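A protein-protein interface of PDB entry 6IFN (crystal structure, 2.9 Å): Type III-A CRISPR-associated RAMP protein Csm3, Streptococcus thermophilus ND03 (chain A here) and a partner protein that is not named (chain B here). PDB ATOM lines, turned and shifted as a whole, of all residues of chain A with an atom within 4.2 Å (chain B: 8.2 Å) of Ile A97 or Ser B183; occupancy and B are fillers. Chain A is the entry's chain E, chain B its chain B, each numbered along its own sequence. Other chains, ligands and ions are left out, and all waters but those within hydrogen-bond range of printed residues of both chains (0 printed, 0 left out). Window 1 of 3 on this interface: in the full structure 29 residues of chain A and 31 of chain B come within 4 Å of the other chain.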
ATOM      1  N   LYS A  53      12.042  12.501  -6.380  1.00  0.00           N
ATOM      2  CA  LYS A  53      10.913  13.372  -6.182  1.00  0.00           C
ATOM      3  C   LYS A  53      11.047  14.066  -4.833  1.00  0.00           C
ATOM      4  O   LYS A  53      10.993  15.272  -4.750  1.00  0.00           O
ATOM      5  CB  LYS A  53       9.588  12.603  -6.224  1.00  0.00           C
ATOM      6  CG  LYS A  53       8.351  13.475  -6.146  1.00  0.00           C
ATOM      7  CD  LYS A  53       7.049  12.732  -6.250  1.00  0.00           C
ATOM      8  CE  LYS A  53       5.865  13.652  -6.032  1.00  0.00           C
ATOM      9  NZ  LYS A  53       4.593  12.895  -6.043  1.00  0.00           N
ATOM     10  N   MET A  93      -3.304  15.216  -7.713  1.00  0.00           N
ATOM     11  CA  MET A  93      -2.087  14.666  -8.335  1.00  0.00           C
ATOM     12  C   MET A  93      -1.339  15.792  -9.051  1.00  0.00           C
ATOM     13  O   MET A  93      -1.897  16.515  -9.858  1.00  0.00           O
ATOM     14  CB  MET A  93      -2.451  13.585  -9.345  1.00  0.00           C
ATOM     15  CG  MET A  93      -2.746  12.264  -8.702  1.00  0.00           C
ATOM     16  SD  MET A  93      -2.254  10.978  -9.851  1.00  0.00           S
ATOM     17  CE  MET A  93      -0.496  10.987  -9.513  1.00  0.00           C
ATOM     18  N   LEU A  96       3.764  15.916 -12.467  1.00  0.00           N
ATOM     19  CA  LEU A  96       5.035  15.199 -12.676  1.00  0.00           C
ATOM     20  C   LEU A  96       4.855  13.716 -12.364  1.00  0.00           C
ATOM     21  O   LEU A  96       4.205  13.365 -11.394  1.00  0.00           O
ATOM     22  CB  LEU A  96       6.110  15.798 -11.768  1.00  0.00           C
ATOM     23  CG  LEU A  96       6.582  17.198 -12.149  1.00  0.00           C
ATOM     24  CD1 LEU A  96       7.459  17.784 -11.070  1.00  0.00           C
ATOM     25  CD2 LEU A  96       7.308  17.210 -13.491  1.00  0.00           C
ATOM     26  N   ILE A  97       5.470  12.864 -13.183  1.00  0.00           N
ATOM     27  CA  ILE A  97       5.526  11.441 -12.944  1.00  0.00           C
ATOM     28  C   ILE A  97       7.001  11.029 -12.986  1.00  0.00           C
ATOM     29  O   ILE A  97       7.607  11.007 -14.070  1.00  0.00           O
ATOM     30  CB  ILE A  97       4.701  10.680 -14.000  1.00  0.00           C
ATOM     31  CG1 ILE A  97       3.210  11.030 -13.948  1.00  0.00           C
ATOM     32  CG2 ILE A  97       4.932   9.184 -13.885  1.00  0.00           C
ATOM     33  CD1 ILE A  97       2.522  10.704 -12.640  1.00  0.00           C
ATOM     34  N   PHE A  98       7.564  10.710 -11.809  1.00  0.00           N
ATOM     35  CA  PHE A  98       8.917  10.192 -11.687  1.00  0.00           C
ATOM     36  C   PHE A  98       8.947   8.696 -12.024  1.00  0.00           C
ATOM     37  O   PHE A  98       7.933   8.006 -11.937  1.00  0.00           O
ATOM     38  CB  PHE A  98       9.454  10.488 -10.290  1.00  0.00           C
ATOM     39  CG  PHE A  98       9.747  11.952 -10.092  1.00  0.00           C
ATOM     40  CD1 PHE A  98      10.957  12.493 -10.491  1.00  0.00           C
ATOM     41  CD2 PHE A  98       8.788  12.806  -9.586  1.00  0.00           C
ATOM     42  CE1 PHE A  98      11.211  13.845 -10.364  1.00  0.00           C
ATOM     43  CE2 PHE A  98       9.040  14.163  -9.476  1.00  0.00           C
ATOM     44  CZ  PHE A  98      10.260  14.677  -9.840  1.00  0.00           C
ATOM     45  N   ARG A  99      10.120   8.209 -12.435  1.00  0.00           N
ATOM     46  CA  ARG A  99      10.335   6.782 -12.703  1.00  0.00           C
ATOM     47  C   ARG A  99      11.586   6.322 -11.952  1.00  0.00           C
ATOM     48  O   ARG A  99      12.601   7.022 -11.958  1.00  0.00           O
ATOM     49  CB  ARG A  99      10.472   6.548 -14.208  1.00  0.00           C
ATOM     50  CG  ARG A  99      10.333   5.091 -14.614  1.00  0.00           C
ATOM     51  CD  ARG A  99      10.632   4.936 -16.084  1.00  0.00           C
ATOM     52  NE  ARG A  99       9.805   3.935 -16.751  1.00  0.00           N
ATOM     53  CZ  ARG A  99      10.151   3.297 -17.871  1.00  0.00           C
ATOM     54  NH1 ARG A  99      11.365   3.477 -18.381  1.00  0.00           N
ATOM     55  NH2 ARG A  99       9.287   2.480 -18.462  1.00  0.00           N
ATOM     56  N   LEU A 151      11.364  11.515 -16.513  1.00  0.00           N
ATOM     57  CA  LEU A 151      10.369  12.265 -15.758  1.00  0.00           C
ATOM     58  C   LEU A 151       9.326  12.790 -16.753  1.00  0.00           C
ATOM     59  O   LEU A 151       9.689  13.329 -17.769  1.00  0.00           O
ATOM     60  CB  LEU A 151      11.090  13.403 -15.018  1.00  0.00           C
ATOM     61  CG  LEU A 151      10.195  14.517 -14.460  1.00  0.00           C
ATOM     62  CD1 LEU A 151       9.378  13.981 -13.301  1.00  0.00           C
ATOM     63  CD2 LEU A 151      10.986  15.755 -14.055  1.00  0.00           C
ATOM     64  N   ILE A 152       8.041  12.657 -16.436  1.00  0.00           N
ATOM     65  CA  ILE A 152       6.988  13.063 -17.342  1.00  0.00           C
ATOM     66  C   ILE A 152       6.292  14.312 -16.803  1.00  0.00           C
ATOM     67  O   ILE A 152       5.917  14.378 -15.641  1.00  0.00           O
ATOM     68  CB  ILE A 152       5.980  11.923 -17.508  1.00  0.00           C
ATOM     69  CG1 ILE A 152       6.644  10.619 -17.979  1.00  0.00           C
ATOM     70  CG2 ILE A 152       4.829  12.372 -18.389  1.00  0.00           C
ATOM     71  CD1 ILE A 152       7.382  10.692 -19.270  1.00  0.00           C
ATOM     72  N   GLU B  39      -8.081   9.625 -17.722  1.00  0.00           N
ATOM     73  CA  GLU B  39      -7.225  10.176 -18.735  1.00  0.00           C
ATOM     74  C   GLU B  39      -8.085  10.920 -19.748  1.00  0.00           C
ATOM     75  O   GLU B  39      -7.732  12.007 -20.186  1.00  0.00           O
ATOM     76  CB  GLU B  39      -6.362   9.132 -19.425  1.00  0.00           C
ATOM     77  CG  GLU B  39      -5.097   8.796 -18.651  1.00  0.00           C
ATOM     78  CD  GLU B  39      -3.867   9.680 -18.845  1.00  0.00           C
ATOM     79  OE1 GLU B  39      -3.334  10.164 -17.846  1.00  0.00           O
ATOM     80  OE2 GLU B  39      -3.416   9.850 -19.984  1.00  0.00           O
ATOM     81  N   LYS B  42      -8.900  14.563 -18.692  1.00  0.00           N
ATOM     82  CA  LYS B  42      -7.988  15.717 -18.806  1.00  0.00           C
ATOM     83  C   LYS B  42      -7.671  15.973 -20.277  1.00  0.00           C
ATOM     84  O   LYS B  42      -7.259  17.065 -20.642  1.00  0.00           O
ATOM     85  CB  LYS B  42      -6.691  15.505 -18.026  1.00  0.00           C
ATOM     86  CG  LYS B  42      -6.187  14.072 -18.015  1.00  0.00           C
ATOM     87  CD  LYS B  42      -4.916  13.911 -17.242  1.00  0.00           C
ATOM     88  CE  LYS B  42      -4.763  12.509 -16.711  1.00  0.00           C
ATOM     89  NZ  LYS B  42      -3.380  12.262 -16.249  1.00  0.00           N
ATOM     90  N   LEU B 173      -1.861   6.789 -21.432  1.00  0.00           N
ATOM     91  CA  LEU B 173      -1.771   6.139 -20.134  1.00  0.00           C
ATOM     92  C   LEU B 173      -0.355   5.601 -19.900  1.00  0.00           C
ATOM     93  O   LEU B 173       0.130   5.608 -18.768  1.00  0.00           O
ATOM     94  CB  LEU B 173      -2.793   5.003 -20.025  1.00  0.00           C
ATOM     95  CG  LEU B 173      -3.973   5.271 -19.095  1.00  0.00           C
ATOM     96  CD1 LEU B 173      -4.769   4.001 -18.857  1.00  0.00           C
ATOM     97  CD2 LEU B 173      -3.507   5.846 -17.760  1.00  0.00           C
ATOM     98  N   GLN B 174       0.338   5.195 -20.965  1.00  0.00           N
ATOM     99  CA  GLN B 174       1.635   4.572 -20.805  1.00  0.00           C
ATOM    100  C   GLN B 174       2.685   5.579 -20.272  1.00  0.00           C
ATOM    101  O   GLN B 174       3.787   5.193 -19.939  1.00  0.00           O
ATOM    102  CB  GLN B 174       2.003   3.840 -22.105  1.00  0.00           C
ATOM    103  CG  GLN B 174       2.455   4.705 -23.276  1.00  0.00           C
ATOM    104  CD  GLN B 174       2.814   3.882 -24.502  1.00  0.00           C
ATOM    105  OE1 GLN B 174       2.886   2.645 -24.486  1.00  0.00           O
ATOM    106  NE2 GLN B 174       3.076   4.578 -25.597  1.00  0.00           N
ATOM    107  N   TYR B 175       2.340   6.863 -20.165  1.00  0.00           N
ATOM    108  CA  TYR B 175       3.170   7.857 -19.449  1.00  0.00           C
ATOM    109  C   TYR B 175       2.499   8.342 -18.155  1.00  0.00           C
ATOM    110  O   TYR B 175       3.079   9.194 -17.443  1.00  0.00           O
ATOM    111  CB  TYR B 175       3.433   9.072 -20.339  1.00  0.00           C
ATOM    112  CG  TYR B 175       4.022   8.682 -21.662  1.00  0.00           C
ATOM    113  CD1 TYR B 175       3.225   8.308 -22.726  1.00  0.00           C
ATOM    114  CD2 TYR B 175       5.397   8.570 -21.790  1.00  0.00           C
ATOM    115  CE1 TYR B 175       3.799   7.884 -23.916  1.00  0.00           C
ATOM    116  CE2 TYR B 175       5.986   8.164 -22.973  1.00  0.00           C
ATOM    117  CZ  TYR B 175       5.183   7.814 -24.040  1.00  0.00           C
ATOM    118  OH  TYR B 175       5.818   7.398 -25.173  1.00  0.00           O
ATOM    119  N   SER B 176       1.294   7.844 -17.857  1.00  0.00           N
ATOM    120  CA  SER B 176       0.654   8.183 -16.601  1.00  0.00           C
ATOM    121  C   SER B 176       0.893   7.099 -15.561  1.00  0.00           C
ATOM    122  O   SER B 176       0.812   7.384 -14.361  1.00  0.00           O
ATOM    123  CB  SER B 176      -0.803   8.433 -16.765  1.00  0.00           C
ATOM    124  OG  SER B 176      -1.037   9.828 -16.843  1.00  0.00           O
ATOM    125  N   GLY B 177       1.142   5.883 -16.045  1.00  0.00           N
ATOM    126  CA  GLY B 177       1.308   4.680 -15.193  1.00  0.00           C
ATOM    127  C   GLY B 177      -0.039   4.049 -14.882  1.00  0.00           C
ATOM    128  O   GLY B 177      -1.066   4.614 -15.292  1.00  0.00           O
ATOM    129  N   LEU B 178      -0.015   2.891 -14.191  1.00  0.00           N
ATOM    130  CA  LEU B 178      -1.222   2.259 -13.635  1.00  0.00           C
ATOM    131  C   LEU B 178      -1.045   1.806 -12.178  1.00  0.00           C
ATOM    132  O   LEU B 178       0.032   1.478 -11.710  1.00  0.00           O
ATOM    133  CB  LEU B 178      -1.627   1.090 -14.523  1.00  0.00           C
ATOM    134  CG  LEU B 178      -2.365   1.501 -15.787  1.00  0.00           C
ATOM    135  CD1 LEU B 178      -2.973   0.292 -16.501  1.00  0.00           C
ATOM    136  CD2 LEU B 178      -3.452   2.508 -15.454  1.00  0.00           C
ATOM    137  N   GLY B 179      -2.184   1.777 -11.486  1.00  0.00           N
ATOM    138  CA  GLY B 179      -2.311   1.503 -10.039  1.00  0.00           C
ATOM    139  C   GLY B 179      -1.521   2.474  -9.190  1.00  0.00           C
ATOM    140  O   GLY B 179      -1.544   3.645  -9.391  1.00  0.00           O
ATOM    141  N   GLY B 180      -0.825   1.940  -8.205  1.00  0.00           N
ATOM    142  CA  GLY B 180       0.551   2.397  -7.947  1.00  0.00           C
ATOM    143  C   GLY B 180       0.610   3.701  -7.190  1.00  0.00           C
ATOM    144  O   GLY B 180      -0.392   4.294  -6.886  1.00  0.00           O
ATOM    145  N   LYS B 181       1.824   4.043  -6.786  1.00  0.00           N
ATOM    146  CA  LYS B 181       2.210   5.382  -6.508  1.00  0.00           C
ATOM    147  C   LYS B 181       2.900   5.880  -7.775  1.00  0.00           C
ATOM    148  O   LYS B 181       4.073   5.789  -7.902  1.00  0.00           O
ATOM    149  CB  LYS B 181       3.129   5.433  -5.285  1.00  0.00           C
ATOM    150  CG  LYS B 181       2.550   4.729  -4.060  1.00  0.00           C
ATOM    151  CD  LYS B 181       3.153   5.182  -2.739  1.00  0.00           C
ATOM    152  CE  LYS B 181       2.237   6.019  -1.875  1.00  0.00           C
ATOM    153  NZ  LYS B 181       2.927   7.252  -1.433  1.00  0.00           N
ATOM    154  N   ARG B 182       2.114   6.361  -8.728  1.00  0.00           N
ATOM    155  CA  ARG B 182       2.602   6.663 -10.046  1.00  0.00           C
ATOM    156  C   ARG B 182       3.503   7.914 -10.007  1.00  0.00           C
ATOM    157  O   ARG B 182       4.581   7.909 -10.532  1.00  0.00           O
ATOM    158  CB  ARG B 182       1.385   6.824 -10.960  1.00  0.00           C
ATOM    159  CG  ARG B 182       0.391   5.667 -10.937  1.00  0.00           C
ATOM    160  CD  ARG B 182      -1.015   6.131 -11.325  1.00  0.00           C
ATOM    161  NE  ARG B 182      -1.002   7.235 -12.277  1.00  0.00           N
ATOM    162  CZ  ARG B 182      -1.782   8.296 -12.204  1.00  0.00           C
ATOM    163  NH1 ARG B 182      -2.927   8.236 -11.544  1.00  0.00           N
ATOM    164  NH2 ARG B 182      -1.399   9.411 -12.807  1.00  0.00           N
ATOM    165  N   SER B 183       3.030   8.995  -9.394  1.00  0.00           N
ATOM    166  CA  SER B 183       3.828  10.153  -9.095  1.00  0.00           C
ATOM    167  C   SER B 183       5.245   9.744  -8.677  1.00  0.00           C
ATOM    168  O   SER B 183       6.218  10.302  -9.188  1.00  0.00           O
ATOM    169  CB  SER B 183       3.173  10.945  -7.999  1.00  0.00           C
ATOM    170  N   SER B 184       5.312   8.758  -7.758  1.00  0.00           N
ATOM    171  CA  SER B 184       6.519   8.310  -6.982  1.00  0.00           C
ATOM    172  C   SER B 184       7.271   7.146  -7.653  1.00  0.00           C
ATOM    173  O   SER B 184       8.003   6.433  -6.981  1.00  0.00           O
ATOM    174  CB  SER B 184       6.123   7.916  -5.562  1.00  0.00           C
ATOM    175  N   GLY B 185       7.080   6.894  -8.946  1.00  0.00           N
ATOM    176  CA  GLY B 185       7.991   5.972  -9.620  1.00  0.00           C
ATOM    177  C   GLY B 185       7.361   4.731 -10.242  1.00  0.00           C
ATOM    178  O   GLY B 185       7.964   4.098 -11.121  1.00  0.00           O
ATOM    179  N   PHE B 186       6.163   4.328  -9.824  1.00  0.00           N
ATOM    180  CA  PHE B 186       5.677   3.020 -10.295  1.00  0.00           C
ATOM    181  C   PHE B 186       4.759   3.169 -11.514  1.00  0.00           C
ATOM    182  O   PHE B 186       4.468   4.291 -11.980  1.00  0.00           O
ATOM    183  CB  PHE B 186       5.092   2.244  -9.113  1.00  0.00           C
ATOM    184  CG  PHE B 186       6.025   2.183  -7.914  1.00  0.00           C
ATOM    185  CD1 PHE B 186       7.333   1.717  -8.039  1.00  0.00           C
ATOM    186  CD2 PHE B 186       5.616   2.615  -6.667  1.00  0.00           C
ATOM    187  CE1 PHE B 186       8.197   1.674  -6.957  1.00  0.00           C
ATOM    188  CE2 PHE B 186       6.482   2.580  -5.587  1.00  0.00           C
ATOM    189  CZ  PHE B 186       7.762   2.101  -5.730  1.00  0.00           C
ATOM    190  N   GLY B 187       4.454   2.017 -12.116  1.00  0.00           N
ATOM    191  CA  GLY B 187       3.313   1.853 -12.981  1.00  0.00           C
ATOM    192  C   GLY B 187       3.521   2.117 -14.473  1.00  0.00           C
ATOM    193  O   GLY B 187       2.731   1.595 -15.244  1.00  0.00           O
ATOM    194  N   ARG B 188       4.476   2.959 -14.900  1.00  0.00           N
ATOM    195  CA  ARG B 188       4.598   3.290 -16.327  1.00  0.00           C
ATOM    196  C   ARG B 188       4.765   1.999 -17.117  1.00  0.00           C
ATOM    197  O   ARG B 188       5.180   0.993 -16.587  1.00  0.00           O
ATOM    198  CB  ARG B 188       5.786   4.199 -16.632  1.00  0.00           C
ATOM    199  CG  ARG B 188       5.774   5.476 -15.808  1.00  0.00           C
ATOM    200  CD  ARG B 188       5.895   6.760 -16.627  1.00  0.00           C
ATOM    201  NE  ARG B 188       7.147   6.937 -17.369  1.00  0.00           N
ATOM    202  CZ  ARG B 188       7.364   6.551 -18.628  1.00  0.00           C
ATOM    203  NH1 ARG B 188       6.417   5.907 -19.320  1.00  0.00           N
ATOM    204  NH2 ARG B 188       8.530   6.860 -19.178  1.00  0.00           N
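Ile A97 touches just these residues of chain B: Tyr B175, Arg B182, Ser B183 and Arg B188. Printed residues of chain A within 4 Å of Tyr B175: Ile A97 and Ile A152. Printed residues of chain A within 4 Å of Arg B188: Ile A97 and Ile A152. The nearest residue of chain B that does not touch Ile A97 is Ser B176 (4.1 Å). The nearest printed residue of chain A that does not touch Ser B183 is Arg A99 (5.5 Å). The nearest printed residue of chain B that does not touch Arg A99 is Arg B188 (4.01 Å).
Hydrophobic or aromatic side chains of chain A that line the printed part of chain B: Met A93, Ile A97, Phe A98 and Ile A152. Along chain A the printed residues that touch a printed residue of chain B span positions 53 to 152. Hydrophobic or aromatic side chains of chain B within 4 Å of the printed part of chain A: Tyr B175. Among the printed residues, no Asp or Glu carboxylate lies within 4 Å of a Lys or Arg side-chain nitrogen of the other chain.
N of Ile A152 sits at hydrogen-bond distance from O of Ile A97 (2.9 Å). The guanidinium group (NE) of Arg B182 is in hydrogen-bond range of the backbone carbonyl oxygen (O) of Ser B176 (2.8 Å). O of Gln B174 lies within hydrogen-bond range of NH1 of Arg B188, 2.8 Å away.
The side-chain sulfur of Met A93 sits at hydrogen-bond distance from the guanidinium group of Arg B182 (3.3 Å). The backbone NH of Phe A98 lies within hydrogen-bond range of the backbone carbonyl oxygen of Ser B183 (3.0 Å). The backbone carbonyl oxygen (O) of Phe A98 lies close to the backbone NH (N) of Gly B185 (3.3 Å).
CB of Ser B183 touches NZ of Lys A53 (3.1 Å). Ser B183 touches Met A93 (CB to CE, 3.97 Å). Ser B183 touches Leu A96 (CA to O, 3.97 Å). Tyr B175 touches Ile A97 (O to CG1, 3.95 Å). CG2 of Ile A97 touches O of Arg B182, at 3.6 Å. Ser B183 touches Ile A97. Arg B188 touches Ile A97 (CD to CG2, 3.8 Å). O of Phe A98 touches O of Arg B182, at 3.6 Å. Tyr B175 touches Ile A152 (O to CG2, 3.7 Å). Ile A152 touches Arg B188 (CG1 to NE, 3.8 Å).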
